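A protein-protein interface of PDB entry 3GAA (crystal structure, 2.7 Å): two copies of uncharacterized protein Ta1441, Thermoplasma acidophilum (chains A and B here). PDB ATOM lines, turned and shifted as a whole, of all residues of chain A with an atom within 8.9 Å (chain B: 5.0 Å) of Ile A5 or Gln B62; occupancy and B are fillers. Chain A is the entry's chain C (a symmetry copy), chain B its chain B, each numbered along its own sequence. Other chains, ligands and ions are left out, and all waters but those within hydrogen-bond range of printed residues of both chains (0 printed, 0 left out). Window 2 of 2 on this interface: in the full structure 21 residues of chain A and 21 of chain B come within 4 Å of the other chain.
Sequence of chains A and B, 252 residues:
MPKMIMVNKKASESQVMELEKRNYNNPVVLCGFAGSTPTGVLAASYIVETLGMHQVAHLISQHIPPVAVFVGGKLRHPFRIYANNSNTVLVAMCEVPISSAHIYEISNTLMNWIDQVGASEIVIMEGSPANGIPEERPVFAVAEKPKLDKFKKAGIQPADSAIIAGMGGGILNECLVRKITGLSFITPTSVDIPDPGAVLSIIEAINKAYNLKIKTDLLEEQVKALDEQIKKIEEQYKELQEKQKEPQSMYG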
ATOM      1  N   MET A   4     -11.302   7.516  11.293  1.00  0.00           N
ATOM      2  CA  MET A   4     -12.319   8.600  11.478  1.00  0.00           C
ATOM      3  C   MET A   4     -12.347   9.562  10.242  1.00  0.00           C
ATOM      4  O   MET A   4     -13.418   9.846   9.707  1.00  0.00           O
ATOM      5  CB  MET A   4     -12.089   9.396  12.809  1.00  0.00           C
ATOM      6  CG  MET A   4     -11.015   8.831  13.886  1.00  0.00           C
ATOM      7  SD  MET A   4     -11.356   7.502  15.199  1.00  0.00           S
ATOM      8  CE  MET A   4     -10.174   7.915  16.534  1.00  0.00           C
ATOM      9  N   ILE A   5     -11.178  10.024   9.787  1.00  0.00           N
ATOM     10  CA  ILE A   5     -11.038  11.092   8.758  1.00  0.00           C
ATOM     11  C   ILE A   5     -10.013  10.768   7.625  1.00  0.00           C
ATOM     12  O   ILE A   5      -8.887  11.180   7.660  1.00  0.00           O
ATOM     13  CB  ILE A   5     -10.673  12.475   9.460  1.00  0.00           C
ATOM     14  CG1 ILE A   5     -11.962  13.185  10.035  1.00  0.00           C
ATOM     15  CG2 ILE A   5      -9.887  13.395   8.511  1.00  0.00           C
ATOM     16  CD1 ILE A   5     -12.544  12.668  11.434  1.00  0.00           C
ATOM     17  N   MET A   6     -10.454  10.066   6.599  1.00  0.00           N
ATOM     18  CA  MET A   6      -9.575   9.384   5.644  1.00  0.00           C
ATOM     19  C   MET A   6      -9.378  10.163   4.323  1.00  0.00           C
ATOM     20  O   MET A   6      -9.892  11.232   4.075  1.00  0.00           O
ATOM     21  CB  MET A   6     -10.090   7.898   5.350  1.00  0.00           C
ATOM     22  CG  MET A   6     -11.747   7.565   5.323  1.00  0.00           C
ATOM     23  SD  MET A   6     -12.479   6.055   4.397  1.00  0.00           S
ATOM     24  CE  MET A   6     -14.249   6.287   4.510  1.00  0.00           C
ATOM     25  N   VAL A   7      -8.644   9.529   3.449  1.00  0.00           N
ATOM     26  CA  VAL A   7      -8.465   9.947   2.091  1.00  0.00           C
ATOM     27  C   VAL A   7      -9.008   8.854   1.191  1.00  0.00           C
ATOM     28  O   VAL A   7      -9.042   7.723   1.562  1.00  0.00           O
ATOM     29  CB  VAL A   7      -7.007   9.994   1.848  1.00  0.00           C
ATOM     30  CG1 VAL A   7      -6.687  10.959   0.670  1.00  0.00           C
ATOM     31  CG2 VAL A   7      -6.256  10.340   3.228  1.00  0.00           C
ATOM     32  N   ASN A   8      -9.400   9.145  -0.020  1.00  0.00           N
ATOM     33  CA  ASN A   8     -10.354   8.243  -0.605  1.00  0.00           C
ATOM     34  C   ASN A   8     -10.312   7.997  -2.071  1.00  0.00           C
ATOM     35  O   ASN A   8     -10.549   8.932  -2.837  1.00  0.00           O
ATOM     36  CB  ASN A   8     -11.674   8.824  -0.293  1.00  0.00           C
ATOM     37  CG  ASN A   8     -12.505   7.866   0.299  1.00  0.00           C
ATOM     38  OD1 ASN A   8     -12.822   6.874  -0.358  1.00  0.00           O
ATOM     39  ND2 ASN A   8     -12.829   8.053   1.593  1.00  0.00           N
ATOM     40  N   ILE B  60     -11.565  13.288   2.832  1.00  0.00           N
ATOM     41  CA  ILE B  60     -12.785  13.337   3.568  1.00  0.00           C
ATOM     42  C   ILE B  60     -12.433  13.620   5.046  1.00  0.00           C
ATOM     43  O   ILE B  60     -11.481  13.088   5.594  1.00  0.00           O
ATOM     44  CB  ILE B  60     -13.583  12.009   3.245  1.00  0.00           C
ATOM     45  CG1 ILE B  60     -14.898  12.370   2.505  1.00  0.00           C
ATOM     46  CG2 ILE B  60     -13.667  11.013   4.446  1.00  0.00           C
ATOM     47  CD1 ILE B  60     -15.645  13.865   2.900  1.00  0.00           C
ATOM     48  N   SER B  61     -13.166  14.516   5.674  1.00  0.00           N
ATOM     49  CA  SER B  61     -12.869  14.900   7.046  1.00  0.00           C
ATOM     50  C   SER B  61     -13.951  15.794   7.571  1.00  0.00           C
ATOM     51  O   SER B  61     -14.454  16.687   6.887  1.00  0.00           O
ATOM     52  CB  SER B  61     -11.563  15.704   7.149  1.00  0.00           C
ATOM     53  OG  SER B  61     -11.330  16.271   8.457  1.00  0.00           O
ATOM     54  N   GLN B  62     -14.260  15.596   8.830  1.00  0.00           N
ATOM     55  CA  GLN B  62     -15.109  16.489   9.539  1.00  0.00           C
ATOM     56  C   GLN B  62     -14.654  17.927   9.489  1.00  0.00           C
ATOM     57  O   GLN B  62     -15.433  18.812   9.757  1.00  0.00           O
ATOM     58  CB  GLN B  62     -15.033  16.065  10.955  1.00  0.00           C
ATOM     59  CG  GLN B  62     -16.103  16.616  11.852  1.00  0.00           C
ATOM     60  CD  GLN B  62     -15.791  16.242  13.280  1.00  0.00           C
ATOM     61  OE1 GLN B  62     -15.088  15.236  13.545  1.00  0.00           O
ATOM     62  NE2 GLN B  62     -16.241  17.079  14.214  1.00  0.00           N
ATOM     63  N   HIS B  63     -13.396  18.175   9.171  1.00  0.00           N
ATOM     64  CA  HIS B  63     -12.846  19.534   9.258  1.00  0.00           C
ATOM     65  C   HIS B  63     -12.601  20.217   7.909  1.00  0.00           C
ATOM     66  O   HIS B  63     -11.857  21.159   7.814  1.00  0.00           O
ATOM     67  CB  HIS B  63     -11.567  19.475  10.070  1.00  0.00           C
ATOM     68  CG  HIS B  63     -11.805  19.001  11.468  1.00  0.00           C
ATOM     69  ND1 HIS B  63     -11.273  17.825  11.964  1.00  0.00           N
ATOM     70  CD2 HIS B  63     -12.589  19.514  12.451  1.00  0.00           C
ATOM     71  CE1 HIS B  63     -11.670  17.669  13.215  1.00  0.00           C
ATOM     72  NE2 HIS B  63     -12.464  18.684  13.533  1.00  0.00           N
ATOM     73  N   ILE B  64     -13.202  19.703   6.863  1.00  0.00           N
ATOM     74  CA  ILE B  64     -13.333  20.419   5.630  1.00  0.00           C
ATOM     75  C   ILE B  64     -14.771  20.927   5.728  1.00  0.00           C
ATOM     76  O   ILE B  64     -15.693  20.184   6.071  1.00  0.00           O
ATOM     77  CB  ILE B  64     -13.052  19.463   4.398  1.00  0.00           C
ATOM     78  CG1 ILE B  64     -11.570  19.017   4.445  1.00  0.00           C
ATOM     79  CG2 ILE B  64     -13.411  20.131   3.082  1.00  0.00           C
ATOM     80  CD1 ILE B  64     -11.215  17.783   3.672  1.00  0.00           C
ATOM     81  N   GLU B 105      -4.499  18.646  11.139  1.00  0.00           N
ATOM     82  CA  GLU B 105      -5.135  17.403  10.845  1.00  0.00           C
ATOM     83  C   GLU B 105      -5.376  17.318   9.331  1.00  0.00           C
ATOM     84  O   GLU B 105      -5.041  16.317   8.683  1.00  0.00           O
ATOM     85  CB  GLU B 105      -6.409  17.218  11.674  1.00  0.00           C
ATOM     86  CG  GLU B 105      -7.742  17.075  10.866  1.00  0.00           C
ATOM     87  CD  GLU B 105      -8.679  15.838  11.289  1.00  0.00           C
ATOM     88  OE1 GLU B 105      -8.494  14.732  10.685  1.00  0.00           O
ATOM     89  OE2 GLU B 105      -9.621  15.988  12.167  1.00  0.00           O
ATOM     90  N   THR B 109      -3.790  14.180   7.270  1.00  0.00           N
ATOM     91  CA  THR B 109      -4.492  13.261   6.438  1.00  0.00           C
ATOM     92  C   THR B 109      -3.913  13.293   5.050  1.00  0.00           C
ATOM     93  O   THR B 109      -3.703  12.269   4.419  1.00  0.00           O
ATOM     94  CB  THR B 109      -5.967  13.660   6.332  1.00  0.00           C
ATOM     95  OG1 THR B 109      -6.576  13.592   7.625  1.00  0.00           O
ATOM     96  CG2 THR B 109      -6.696  12.777   5.359  1.00  0.00           C
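O of Met A6 is in hydrogen-bond range of N of Ile B60, at 2.9 Å.
O of Ile A5 is in hydrogen-bond range of OG1 of Thr B109 (3.3 Å).
The side-chain hydroxyl (OG) of Ser B61 is in hydrogen-bond range of the backbone NH (N) of His B63.
The side-chain carboxylate (OE2) of Glu B105 is in hydrogen-bond range of a ring nitrogen (ND1) of His B63, at 2.5 Å.
The backbone carbonyl oxygen (O) of Glu B105 lies within hydrogen-bond range of the side-chain hydroxyl (OG1) of Thr B109 (3.3 Å).
The side-chain amide nitrogen (ND2) of Asn A8 lies within hydrogen-bond range of the side-chain sulfur (SD) of Met A6 (3.5 Å).
Among the printed residues, merely in contact across the chains: Ile A5 with Glu B105 (2.9 Å), Ile A5 with Ser B61 (3.2 Å), Val A7 with Thr B109 (3.3 Å), Ile A5 with Ile B60 (3.3 Å), Ile A5 with Gln B62 (3.5 Å) and Met A6 with Thr B109 (3.8 Å).
Of chain A, only Ile A5 comes within 4 Å of Gln B62.
No residue of chain A comes within 4 Å of His B63.
Printed residues of chain B within 4 Å of Met A6: Ile B60 and Thr B109.
Printed residues of chain A within 4 Å of Thr B109: Ile A5, Met A6 and Val A7.
Printed residues of chain A within 4 Å of Glu B105: Ile A5.
Printed residues of chain B within 4 Å of Val A7: Thr B109.
Of the printed residues of chain A, Ile B60 touches Ile A5 and Met A6.
Ile B64 touches none of the printed residues of chain A.
Met A4 touches none of the printed residues of chain B.
Printed residues of chain A that touch a printed residue of chain B: Ile A5, Met A6 and Val A7.
Hydrophobic or aromatic side chains of chain A that line the printed part of chain B: Ile A5 and Val A7.
Of the 7 printed residues of chain B, 5 touch a printed residue of chain A.
Printed residues of chain B that touch a printed residue of chain A: Ile B60, Ser B61, Gln B62, Glu B105 and Thr B109.
Hydrophobic or aromatic side chains of chain B within 4 Å of the printed part of chain A: Ile B60.
Among the printed residues, 8 pairs touch across the chains.
No position is printed for both chains.
Of the 8 pairs that touch across the chains among the printed residues, none has its exchanged pair printed and touching as well.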
